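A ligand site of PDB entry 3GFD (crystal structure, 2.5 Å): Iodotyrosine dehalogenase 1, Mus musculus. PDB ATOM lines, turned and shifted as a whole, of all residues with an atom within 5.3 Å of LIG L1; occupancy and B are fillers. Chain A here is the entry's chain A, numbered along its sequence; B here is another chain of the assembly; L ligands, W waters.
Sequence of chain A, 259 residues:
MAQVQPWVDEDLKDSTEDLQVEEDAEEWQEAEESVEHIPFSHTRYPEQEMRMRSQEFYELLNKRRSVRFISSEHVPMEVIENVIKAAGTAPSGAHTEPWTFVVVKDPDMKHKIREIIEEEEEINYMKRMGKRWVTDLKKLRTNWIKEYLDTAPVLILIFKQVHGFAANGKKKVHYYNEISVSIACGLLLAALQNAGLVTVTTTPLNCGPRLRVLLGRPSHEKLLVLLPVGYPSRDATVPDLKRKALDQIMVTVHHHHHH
O3 of LIG L1 sits at hydrogen-bond distance from O1 of LG2 L2 (2.5 Å).
Water W4 lies within hydrogen-bond range of O1 of LIG L1 (2.6 Å), OH of Tyr 148 (2.8 Å) and NZ of Lys 146 (2.8 Å).
Water W2 lies within hydrogen-bond range of the guanidinium group of Arg 68 (2.8 Å) and an oxygen (O5) of LIG L1 (2.9 Å).
Water W5 lies within hydrogen-bond range of O of Ser 66 (2.8 Å), O7 of LIG L1 (2.9 Å) and NH2 of Arg 65 (3.2 Å).
Water W3 lies within hydrogen-bond range of the side-chain hydroxyl of Ser 92 of chain B and a ring nitrogen (ND1) of His 95 of chain B.
N4 of LIG L1 lies close to O of Thr 201 (2.8 Å).
Leu 140 touches LIG L1 (CD1 to O5, 3.7 Å).
Thr 142 touches LIG L1.
CG2 of Val 200 touches N1 of LIG L1 (3.4 Å).
Thr 202 touches LIG L1 (CA to O2, 3.7 Å).
CD1 of Leu 241 touches O5 of LIG L1, 3.7 Å away.
CB of Pro 91 of chain B touches O4 of LIG L1, 3.1 Å away.
Gly 93 of chain B touches LIG L1.
Ala 94 of chain B touches LIG L1.
N of His 95 of chain B touches C16 of LIG L1, at 3.7 Å.
Tyr 176 of chain B touches LIG L1.
Ile 179 of chain B touches LIG L1 (CG2 to C7, 3.996 Å).
Ser 180 of chain B touches LIG L1 (OG to C9, 3.8 Å).
Of the 28 residues printed, 20 come within 4 Å of LIG L1.
Along chain A the residues within 4 Å of LIG L1 span positions 64 to 243.
The nearest printed residue that does not touch LIG L1 is Ile 183 of chain B (4.1 Å).
NH2 of Arg 243 lies within hydrogen-bond range of O of Arg 64, at 2.9 Å.
NH2 of Arg 243 is in hydrogen-bond range of O of Thr 89 of chain B, 3.4 Å away.
O of Thr 89 of chain B is in hydrogen-bond range of NH2 of Arg 64, 2.8 Å away.
N of Gly 93 of chain B lies within hydrogen-bond range of OG of Ser 180 of chain B (3.2 Å).
OG of Ser 180 of chain B lies within hydrogen-bond range of O of Tyr 176 of chain B, at 2.8 Å.
O1 of LIG L1 lies within hydrogen-bond range of NE of Arg 68, 2.6 Å away.
The backbone NH (N) of Ser 66 is in hydrogen-bond range of an oxygen (O7) of LIG L1, 2.8 Å away.
The side-chain hydroxyl (OG) of Ser 66 lies within hydrogen-bond range of an oxygen (O8) of LIG L1 (2.6 Å).
An oxygen (O7) of LIG L1 is in salt-bridge range of the guanidinium group (NE) of Arg 65 (2.7 Å).
NH2 of Arg 243 is in salt-bridge range of O9 of LIG L1 (2.8 Å).
An oxygen (O2) of LIG L1 lies within hydrogen-bond range of the backbone NH of Thr 203.
The side-chain hydroxyl (OG1) of Thr 203 is in hydrogen-bond range of a nitrogen (N3) of LIG L1 (3.1 Å).
An oxygen (O8) of LIG L1 lies within salt-bridge range of the guanidinium group of Arg 64.
The backbone NH of Ser 92 of chain B sits at hydrogen-bond distance from an oxygen (O4) of LIG L1, at 3.3 Å.
A nitrogen (N1) of LG2 L2 lies within hydrogen-bond range of the backbone carbonyl oxygen (O) of Thr 203, at 3.4 Å.
The backbone NH (N) of Ala 94 of chain B sits at hydrogen-bond distance from an oxygen (O1) of LG2 L2 (2.8 Å).
The side-chain amino group of Lys 146 is in salt-bridge range of an oxygen (O3) of LG2 L2, 2.8 Å away.
A nitrogen (N1) of LG2 L2 lies within salt-bridge range of the side-chain carboxylate (OE2) of Glu 121, 2.8 Å away.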
ATOM      1  N   ARG A  64      23.368  17.859 -15.052  1.00  0.00           N
ATOM      2  CA  ARG A  64      22.250  18.825 -14.924  1.00  0.00           C
ATOM      3  C   ARG A  64      20.962  18.140 -15.323  1.00  0.00           C
ATOM      4  O   ARG A  64      20.904  17.493 -16.394  1.00  0.00           O
ATOM      5  CB  ARG A  64      22.463  20.041 -15.829  1.00  0.00           C
ATOM      6  CG  ARG A  64      21.415  21.152 -15.700  1.00  0.00           C
ATOM      7  CD  ARG A  64      21.329  21.984 -17.017  1.00  0.00           C
ATOM      8  NE  ARG A  64      20.868  21.114 -18.097  1.00  0.00           N
ATOM      9  CZ  ARG A  64      19.632  20.602 -18.173  1.00  0.00           C
ATOM     10  NH1 ARG A  64      18.690  20.976 -17.247  1.00  0.00           N
ATOM     11  NH2 ARG A  64      19.322  19.748 -19.173  1.00  0.00           N
ATOM     12  N   ARG A  65      19.956  18.241 -14.463  1.00  0.00           N
ATOM     13  CA  ARG A  65      18.577  17.875 -14.827  1.00  0.00           C
ATOM     14  C   ARG A  65      17.654  19.018 -14.407  1.00  0.00           C
ATOM     15  O   ARG A  65      17.930  19.757 -13.435  1.00  0.00           O
ATOM     16  CB  ARG A  65      18.139  16.589 -14.113  1.00  0.00           C
ATOM     17  CG  ARG A  65      18.923  15.310 -14.536  1.00  0.00           C
ATOM     18  CD  ARG A  65      18.791  14.978 -16.031  1.00  0.00           C
ATOM     19  NE  ARG A  65      17.382  14.914 -16.396  1.00  0.00           N
ATOM     20  CZ  ARG A  65      16.618  13.835 -16.250  1.00  0.00           C
ATOM     21  NH1 ARG A  65      17.116  12.689 -15.773  1.00  0.00           N
ATOM     22  NH2 ARG A  65      15.336  13.895 -16.579  1.00  0.00           N
ATOM     23  N   SER A  66      16.563  19.195 -15.137  1.00  0.00           N
ATOM     24  CA  SER A  66      15.551  20.131 -14.686  1.00  0.00           C
ATOM     25  C   SER A  66      14.903  19.546 -13.415  1.00  0.00           C
ATOM     26  O   SER A  66      14.354  18.439 -13.455  1.00  0.00           O
ATOM     27  CB  SER A  66      14.519  20.355 -15.792  1.00  0.00           C
ATOM     28  OG  SER A  66      15.147  21.080 -16.847  1.00  0.00           O
ATOM     29  N   ARG A  68      12.178  20.056 -10.345  1.00  0.00           N
ATOM     30  CA  ARG A  68      10.952  20.776 -10.086  1.00  0.00           C
ATOM     31  C   ARG A  68      10.509  20.804  -8.604  1.00  0.00           C
ATOM     32  O   ARG A  68       9.383  21.226  -8.271  1.00  0.00           O
ATOM     33  CB  ARG A  68       9.868  20.208 -10.977  1.00  0.00           C
ATOM     34  CG  ARG A  68      10.166  20.387 -12.452  1.00  0.00           C
ATOM     35  CD  ARG A  68       9.107  19.773 -13.344  1.00  0.00           C
ATOM     36  NE  ARG A  68       9.389  20.157 -14.739  1.00  0.00           N
ATOM     37  CZ  ARG A  68      10.011  19.364 -15.611  1.00  0.00           C
ATOM     38  NH1 ARG A  68      10.399  18.125 -15.259  1.00  0.00           N
ATOM     39  NH2 ARG A  68      10.240  19.779 -16.840  1.00  0.00           N
ATOM     40  N   GLU A 121      -1.537  28.880 -15.881  1.00  0.00           N
ATOM     41  CA  GLU A 121      -1.187  27.522 -16.331  1.00  0.00           C
ATOM     42  C   GLU A 121      -2.398  26.610 -16.325  1.00  0.00           C
ATOM     43  O   GLU A 121      -2.501  25.694 -17.137  1.00  0.00           O
ATOM     44  CB  GLU A 121      -0.070  26.879 -15.495  1.00  0.00           C
ATOM     45  CG  GLU A 121       1.369  27.397 -15.703  1.00  0.00           C
ATOM     46  CD  GLU A 121       1.919  27.213 -17.121  1.00  0.00           C
ATOM     47  OE1 GLU A 121       1.134  26.901 -18.064  1.00  0.00           O
ATOM     48  OE2 GLU A 121       3.159  27.386 -17.291  1.00  0.00           O
ATOM     49  N   LEU A 140       6.364  13.924 -18.217  1.00  0.00           N
ATOM     50  CA  LEU A 140       7.066  14.817 -17.315  1.00  0.00           C
ATOM     51  C   LEU A 140       6.280  14.949 -16.010  1.00  0.00           C
ATOM     52  O   LEU A 140       6.820  15.402 -14.997  1.00  0.00           O
ATOM     53  CB  LEU A 140       7.188  16.160 -18.012  1.00  0.00           C
ATOM     54  CG  LEU A 140       8.412  16.483 -18.866  1.00  0.00           C
ATOM     55  CD1 LEU A 140       9.297  15.336 -19.376  1.00  0.00           C
ATOM     56  CD2 LEU A 140       8.102  17.423 -20.013  1.00  0.00           C
ATOM     57  N   THR A 142       4.131  17.143 -15.227  1.00  0.00           N
ATOM     58  CA  THR A 142       3.944  18.521 -14.769  1.00  0.00           C
ATOM     59  C   THR A 142       2.444  18.865 -14.719  1.00  0.00           C
ATOM     60  O   THR A 142       1.649  18.308 -15.457  1.00  0.00           O
ATOM     61  CB  THR A 142       4.648  19.462 -15.725  1.00  0.00           C
ATOM     62  OG1 THR A 142       4.290  19.072 -17.056  1.00  0.00           O
ATOM     63  CG2 THR A 142       6.160  19.333 -15.574  1.00  0.00           C
ATOM     64  N   LYS A 146       2.633  24.976  -8.858  1.00  0.00           N
ATOM     65  CA  LYS A 146       4.030  25.297  -8.903  1.00  0.00           C
ATOM     66  C   LYS A 146       4.497  25.760  -7.546  1.00  0.00           C
ATOM     67  O   LYS A 146       4.828  26.947  -7.310  1.00  0.00           O
ATOM     68  CB  LYS A 146       4.341  26.374  -9.962  1.00  0.00           C
ATOM     69  CG  LYS A 146       3.870  26.031 -11.345  1.00  0.00           C
ATOM     70  CD  LYS A 146       4.574  24.801 -11.881  1.00  0.00           C
ATOM     71  CE  LYS A 146       4.146  24.539 -13.341  1.00  0.00           C
ATOM     72  NZ  LYS A 146       4.654  23.207 -13.857  1.00  0.00           N
ATOM     73  N   TYR A 148       7.227  25.329  -6.138  1.00  0.00           N
ATOM     74  CA  TYR A 148       8.565  25.905  -6.135  1.00  0.00           C
ATOM     75  C   TYR A 148       8.551  27.455  -6.222  1.00  0.00           C
ATOM     76  O   TYR A 148       9.476  28.083  -5.753  1.00  0.00           O
ATOM     77  CB  TYR A 148       9.492  25.302  -7.228  1.00  0.00           C
ATOM     78  CG  TYR A 148       8.983  25.418  -8.655  1.00  0.00           C
ATOM     79  CD1 TYR A 148       8.564  24.280  -9.361  1.00  0.00           C
ATOM     80  CD2 TYR A 148       8.938  26.660  -9.312  1.00  0.00           C
ATOM     81  CE1 TYR A 148       8.109  24.373 -10.712  1.00  0.00           C
ATOM     82  CE2 TYR A 148       8.506  26.776 -10.636  1.00  0.00           C
ATOM     83  CZ  TYR A 148       8.107  25.637 -11.332  1.00  0.00           C
ATOM     84  OH  TYR A 148       7.648  25.783 -12.633  1.00  0.00           O
ATOM     85  N   VAL A 200      14.777  24.663 -12.927  1.00  0.00           N
ATOM     86  CA  VAL A 200      14.119  24.179 -14.118  1.00  0.00           C
ATOM     87  C   VAL A 200      13.858  25.407 -14.988  1.00  0.00           C
ATOM     88  O   VAL A 200      13.389  26.425 -14.468  1.00  0.00           O
ATOM     89  CB  VAL A 200      12.811  23.367 -13.847  1.00  0.00           C
ATOM     90  CG1 VAL A 200      11.891  24.077 -12.878  1.00  0.00           C
ATOM     91  CG2 VAL A 200      12.087  23.039 -15.174  1.00  0.00           C
ATOM     92  N   THR A 201      14.142  25.296 -16.280  1.00  0.00           N
ATOM     93  CA  THR A 201      13.896  26.394 -17.215  1.00  0.00           C
ATOM     94  C   THR A 201      12.413  26.400 -17.494  1.00  0.00           C
ATOM     95  O   THR A 201      11.896  25.402 -18.036  1.00  0.00           O
ATOM     96  CB  THR A 201      14.648  26.073 -18.562  1.00  0.00           C
ATOM     97  OG1 THR A 201      16.032  25.930 -18.266  1.00  0.00           O
ATOM     98  CG2 THR A 201      14.456  27.164 -19.597  1.00  0.00           C
ATOM     99  N   THR A 202      11.704  27.473 -17.119  1.00  0.00           N
ATOM    100  CA  THR A 202      10.228  27.454 -17.413  1.00  0.00           C
ATOM    101  C   THR A 202       9.792  28.556 -18.360  1.00  0.00           C
ATOM    102  O   THR A 202      10.437  29.594 -18.438  1.00  0.00           O
ATOM    103  CB  THR A 202       9.331  27.421 -16.136  1.00  0.00           C
ATOM    104  OG1 THR A 202       9.366  28.693 -15.491  1.00  0.00           O
ATOM    105  CG2 THR A 202       9.813  26.368 -15.168  1.00  0.00           C
ATOM    106  N   THR A 203       8.724  28.297 -19.091  1.00  0.00           N
ATOM    107  CA  THR A 203       8.097  29.272 -19.983  1.00  0.00           C
ATOM    108  C   THR A 203       6.597  29.328 -19.577  1.00  0.00           C
ATOM    109  O   THR A 203       5.758  28.579 -20.082  1.00  0.00           O
ATOM    110  CB  THR A 203       8.158  28.808 -21.438  1.00  0.00           C
ATOM    111  OG1 THR A 203       7.784  27.417 -21.489  1.00  0.00           O
ATOM    112  CG2 THR A 203       9.546  29.003 -21.999  1.00  0.00           C
ATOM    113  N   PRO A 204       6.253  30.251 -18.689  1.00  0.00           N
ATOM    114  CA  PRO A 204       4.875  30.327 -18.256  1.00  0.00           C
ATOM    115  C   PRO A 204       4.019  31.037 -19.339  1.00  0.00           C
ATOM    116  O   PRO A 204       3.902  32.287 -19.355  1.00  0.00           O
ATOM    117  CB  PRO A 204       4.960  31.156 -16.977  1.00  0.00           C
ATOM    118  CG  PRO A 204       6.392  31.691 -16.914  1.00  0.00           C
ATOM    119  CD  PRO A 204       7.118  31.288 -18.121  1.00  0.00           C
ATOM    120  N   VAL A 225      12.160  33.442 -19.898  1.00  0.00           N
ATOM    121  CA  VAL A 225      12.031  32.244 -19.048  1.00  0.00           C
ATOM    122  C   VAL A 225      12.086  32.596 -17.558  1.00  0.00           C
ATOM    123  O   VAL A 225      12.690  33.608 -17.140  1.00  0.00           O
ATOM    124  CB  VAL A 225      13.190  31.173 -19.306  1.00  0.00           C
ATOM    125  CG1 VAL A 225      13.092  30.517 -20.703  1.00  0.00           C
ATOM    126  CG2 VAL A 225      14.541  31.812 -19.143  1.00  0.00           C
ATOM    127  N   LEU A 241      14.456  10.298 -18.320  1.00  0.00           N
ATOM    128  CA  LEU A 241      14.656  10.587 -19.727  1.00  0.00           C
ATOM    129  C   LEU A 241      16.086  10.231 -20.132  1.00  0.00           C
ATOM    130  O   LEU A 241      17.021  10.273 -19.296  1.00  0.00           O
ATOM    131  CB  LEU A 241      14.416  12.066 -19.965  1.00  0.00           C
ATOM    132  CG  LEU A 241      13.124  12.670 -19.416  1.00  0.00           C
ATOM    133  CD1 LEU A 241      13.079  14.178 -19.627  1.00  0.00           C
ATOM    134  CD2 LEU A 241      11.915  11.984 -20.059  1.00  0.00           C
ATOM    135  N   ARG A 243      19.143  11.090 -23.136  1.00  0.00           N
ATOM    136  CA  ARG A 243      19.574  12.013 -24.162  1.00  0.00           C
ATOM    137  C   ARG A 243      20.044  11.205 -25.359  1.00  0.00           C
ATOM    138  O   ARG A 243      20.522  10.056 -25.209  1.00  0.00           O
ATOM    139  CB  ARG A 243      20.681  12.899 -23.613  1.00  0.00           C
ATOM    140  CG  ARG A 243      20.095  13.912 -22.653  1.00  0.00           C
ATOM    141  CD  ARG A 243      21.138  14.681 -21.865  1.00  0.00           C
ATOM    142  NE  ARG A 243      20.434  15.617 -21.003  1.00  0.00           N
ATOM    143  CZ  ARG A 243      20.824  15.986 -19.799  1.00  0.00           C
ATOM    144  NH1 ARG A 243      21.964  15.511 -19.283  1.00  0.00           N
ATOM    145  NH2 ARG A 243      20.052  16.812 -19.119  1.00  0.00           N
ATOM    146  N   THR B  89      23.480  18.356 -23.795  1.00  0.00           N
ATOM    147  CA  THR B  89      22.927  18.200 -22.429  1.00  0.00           C
ATOM    148  C   THR B  89      21.909  19.300 -22.083  1.00  0.00           C
ATOM    149  O   THR B  89      21.305  19.284 -21.022  1.00  0.00           O
ATOM    150  CB  THR B  89      24.010  18.214 -21.330  1.00  0.00           C
ATOM    151  OG1 THR B  89      24.595  19.529 -21.252  1.00  0.00           O
ATOM    152  CG2 THR B  89      25.093  17.099 -21.601  1.00  0.00           C
ATOM    153  N   ALA B  90      21.716  20.261 -22.999  1.00  0.00           N
ATOM    154  CA  ALA B  90      20.869  21.399 -22.752  1.00  0.00           C
ATOM    155  C   ALA B  90      19.425  20.937 -22.473  1.00  0.00           C
ATOM    156  O   ALA B  90      18.979  19.942 -23.005  1.00  0.00           O
ATOM    157  CB  ALA B  90      20.876  22.273 -23.955  1.00  0.00           C
ATOM    158  N   PRO B  91      18.664  21.719 -21.702  1.00  0.00           N
ATOM    159  CA  PRO B  91      17.227  21.415 -21.599  1.00  0.00           C
ATOM    160  C   PRO B  91      16.563  21.683 -22.947  1.00  0.00           C
ATOM    161  O   PRO B  91      17.114  22.427 -23.761  1.00  0.00           O
ATOM    162  CB  PRO B  91      16.731  22.439 -20.569  1.00  0.00           C
ATOM    163  CG  PRO B  91      17.763  23.629 -20.747  1.00  0.00           C
ATOM    164  CD  PRO B  91      19.077  22.912 -20.935  1.00  0.00           C
ATOM    165  N   SER B  92      15.368  21.134 -23.169  1.00  0.00           N
ATOM    166  CA  SER B  92      14.616  21.470 -24.347  1.00  0.00           C
ATOM    167  C   SER B  92      13.143  21.319 -24.082  1.00  0.00           C
ATOM    168  O   SER B  92      12.696  20.446 -23.271  1.00  0.00           O
ATOM    169  CB  SER B  92      15.029  20.606 -25.554  1.00  0.00           C
ATOM    170  OG  SER B  92      14.687  19.222 -25.351  1.00  0.00           O
ATOM    171  N   GLY B  93      12.355  22.120 -24.776  1.00  0.00           N
ATOM    172  CA  GLY B  93      10.902  22.107 -24.529  1.00  0.00           C
ATOM    173  C   GLY B  93      10.339  20.705 -24.712  1.00  0.00           C
ATOM    174  O   GLY B  93      10.536  20.088 -25.767  1.00  0.00           O
ATOM    175  N   ALA B  94       9.630  20.202 -23.684  1.00  0.00           N
ATOM    176  CA  ALA B  94       9.064  18.825 -23.698  1.00  0.00           C
ATOM    177  C   ALA B  94      10.082  17.717 -24.083  1.00  0.00           C
ATOM    178  O   ALA B  94       9.705  16.702 -24.662  1.00  0.00           O
ATOM    179  CB  ALA B  94       7.792  18.736 -24.589  1.00  0.00           C
ATOM    180  N   HIS B  95      11.365  17.898 -23.733  1.00  0.00           N
ATOM    181  CA  HIS B  95      12.417  16.912 -24.051  1.00  0.00           C
ATOM    182  C   HIS B  95      12.436  16.513 -25.520  1.00  0.00           C
ATOM    183  O   HIS B  95      12.352  15.330 -25.868  1.00  0.00           O
ATOM    184  CB  HIS B  95      12.310  15.663 -23.139  1.00  0.00           C
ATOM    185  CG  HIS B  95      13.446  14.678 -23.293  1.00  0.00           C
ATOM    186  ND1 HIS B  95      14.775  15.054 -23.218  1.00  0.00           N
ATOM    187  CD2 HIS B  95      13.439  13.341 -23.536  1.00  0.00           C
ATOM    188  CE1 HIS B  95      15.540  13.988 -23.419  1.00  0.00           C
ATOM    189  NE2 HIS B  95      14.751  12.939 -23.595  1.00  0.00           N
ATOM    190  N   TYR B 176       9.166  25.547 -28.505  1.00  0.00           N
ATOM    191  CA  TYR B 176      10.211  26.498 -28.235  1.00  0.00           C
ATOM    192  C   TYR B 176      11.550  26.005 -28.817  1.00  0.00           C
ATOM    193  O   TYR B 176      12.587  26.092 -28.143  1.00  0.00           O
ATOM    194  CB  TYR B 176      10.347  26.778 -26.740  1.00  0.00           C
ATOM    195  CG  TYR B 176       9.068  27.208 -26.073  1.00  0.00           C
ATOM    196  CD1 TYR B 176       8.369  26.345 -25.235  1.00  0.00           C
ATOM    197  CD2 TYR B 176       8.588  28.489 -26.231  1.00  0.00           C
ATOM    198  CE1 TYR B 176       7.189  26.744 -24.602  1.00  0.00           C
ATOM    199  CE2 TYR B 176       7.402  28.930 -25.596  1.00  0.00           C
ATOM    200  CZ  TYR B 176       6.702  28.052 -24.786  1.00  0.00           C
ATOM    201  OH  TYR B 176       5.535  28.479 -24.158  1.00  0.00           O
ATOM    202  N   ILE B 179      14.438  28.792 -28.985  1.00  0.00           N
ATOM    203  CA  ILE B 179      15.042  29.050 -27.676  1.00  0.00           C
ATOM    204  C   ILE B 179      15.885  27.847 -27.194  1.00  0.00           C
ATOM    205  O   ILE B 179      17.002  28.031 -26.693  1.00  0.00           O
ATOM    206  CB  ILE B 179      13.988  29.440 -26.652  1.00  0.00           C
ATOM    207  CG1 ILE B 179      13.244  30.728 -27.058  1.00  0.00           C
ATOM    208  CG2 ILE B 179      14.575  29.590 -25.279  1.00  0.00           C
ATOM    209  CD1 ILE B 179      11.911  30.920 -26.332  1.00  0.00           C
ATOM    210  N   SER B 180      15.364  26.621 -27.342  1.00  0.00           N
ATOM    211  CA  SER B 180      16.087  25.416 -26.902  1.00  0.00           C
ATOM    212  C   SER B 180      17.429  25.300 -27.603  1.00  0.00           C
ATOM    213  O   SER B 180      18.476  25.067 -26.975  1.00  0.00           O
ATOM    214  CB  SER B 180      15.271  24.189 -27.256  1.00  0.00           C
ATOM    215  OG  SER B 180      14.016  24.196 -26.573  1.00  0.00           O
ATOM    216  N   ILE B 183      19.775  27.893 -26.285  1.00  0.00           N
ATOM    217  CA  ILE B 183      20.381  27.476 -24.999  1.00  0.00           C
ATOM    218  C   ILE B 183      21.511  26.488 -25.275  1.00  0.00           C
ATOM    219  O   ILE B 183      22.628  26.672 -24.773  1.00  0.00           O
ATOM    220  CB  ILE B 183      19.327  26.930 -24.066  1.00  0.00           C
ATOM    221  CG1 ILE B 183      18.475  28.104 -23.551  1.00  0.00           C
ATOM    222  CG2 ILE B 183      19.946  26.034 -22.946  1.00  0.00           C
ATOM    223  CD1 ILE B 183      17.189  27.660 -22.825  1.00  0.00           C
HETATM  224  N1  LIG L   1       9.703  22.537 -17.570  1.00  0.00           N
HETATM  225  C1  LIG L   1       8.571  22.855 -16.899  1.00  0.00           C
HETATM  226  O1  LIG L   1       8.329  22.215 -15.870  1.00  0.00           O
HETATM  227  N2  LIG L   1       7.755  23.816 -17.340  1.00  0.00           N
HETATM  228  C2  LIG L   1       7.954  24.552 -18.482  1.00  0.00           C
HETATM  229  O2  LIG L   1       7.390  25.588 -18.937  1.00  0.00           O
HETATM  230  C3  LIG L   1       9.117  24.242 -19.144  1.00  0.00           C
HETATM  231  N3  LIG L   1       9.298  24.998 -20.301  1.00  0.00           N
HETATM  232  C4  LIG L   1      10.461  24.829 -20.982  1.00  0.00           C
HETATM  233  C5  LIG L   1      10.714  25.609 -22.072  1.00  0.00           C
HETATM  234  C6  LIG L   1      11.933  25.469 -22.819  1.00  0.00           C
HETATM  235  C7  LIG L   1      12.492  26.554 -23.725  1.00  0.00           C
HETATM  236  C8  LIG L   1      12.890  24.504 -22.407  1.00  0.00           C
HETATM  237  C9  LIG L   1      14.323  24.761 -22.837  1.00  0.00           C
HETATM  238  C10 LIG L   1      12.595  23.721 -21.256  1.00  0.00           C
HETATM  239  C11 LIG L   1      11.397  23.858 -20.558  1.00  0.00           C
HETATM  240  N4  LIG L   1      11.171  23.064 -19.415  1.00  0.00           N
HETATM  241  C12 LIG L   1      10.002  23.272 -18.701  1.00  0.00           C
HETATM  242  C13 LIG L   1      12.232  21.935 -19.121  1.00  0.00           C
HETATM  243  C14 LIG L   1      12.077  20.741 -20.069  1.00  0.00           C
HETATM  244  O3  LIG L   1      10.804  20.173 -19.889  1.00  0.00           O
HETATM  245  C15 LIG L   1      13.191  19.783 -19.759  1.00  0.00           C
HETATM  246  O4  LIG L   1      14.405  20.392 -20.132  1.00  0.00           O
HETATM  247  C16 LIG L   1      13.123  18.461 -20.517  1.00  0.00           C
HETATM  248  O5  LIG L   1      12.022  17.747 -20.030  1.00  0.00           O
HETATM  249  C17 LIG L   1      14.437  17.646 -20.480  1.00  0.00           C
HETATM  250  O6  LIG L   1      14.829  17.541 -19.127  1.00  0.00           O
HETATM  251  P1  LIG L   1      16.276  17.933 -18.595  1.00  0.00           P
HETATM  252  O7  LIG L   1      16.441  17.342 -17.204  1.00  0.00           O
HETATM  253  O8  LIG L   1      16.374  19.462 -18.513  1.00  0.00           O
HETATM  254  O9  LIG L   1      17.368  17.408 -19.499  1.00  0.00           O
HETATM  255  N1  LG2 L   2       4.575  25.609 -18.892  1.00  0.00           N
HETATM  256  C1  LG2 L   2       3.818  24.460 -18.332  1.00  0.00           C
HETATM  257  C2  LG2 L   2       3.869  23.298 -19.285  1.00  0.00           C
HETATM  258  C3  LG2 L   2       5.225  22.750 -19.723  1.00  0.00           C
HETATM  259  C4  LG2 L   2       5.678  23.079 -21.013  1.00  0.00           C
HETATM  260  C5  LG2 L   2       6.902  22.586 -21.524  1.00  0.00           C
HETATM  261  I1  LG2 L   2       7.519  23.065 -23.478  1.00  0.00           I
HETATM  262  C6  LG2 L   2       7.689  21.657 -20.702  1.00  0.00           C
HETATM  263  O1  LG2 L   2       8.862  21.162 -21.203  1.00  0.00           O
HETATM  264  C7  LG2 L   2       7.195  21.322 -19.411  1.00  0.00           C
HETATM  265  C8  LG2 L   2       5.989  21.873 -18.912  1.00  0.00           C
HETATM  266  C9  LG2 L   2       4.341  23.962 -16.999  1.00  0.00           C
HETATM  267  O2  LG2 L   2       5.245  24.551 -16.379  1.00  0.00           O
HETATM  268  O3  LG2 L   2       3.861  22.916 -16.499  1.00  0.00           O
HETATM  269  O   HOH W   1      16.908  14.933 -20.316  1.00  0.00           O
HETATM  270  O   HOH W   2      11.993  17.046 -17.259  1.00  0.00           O
HETATM  271  O   HOH W   3      16.008  17.799 -23.513  1.00  0.00           O
HETATM  272  O   HOH W   4       7.477  23.231 -13.677  1.00  0.00           O
HETATM  273  O   HOH W   5      14.050  16.697 -15.659  1.00  0.00           O
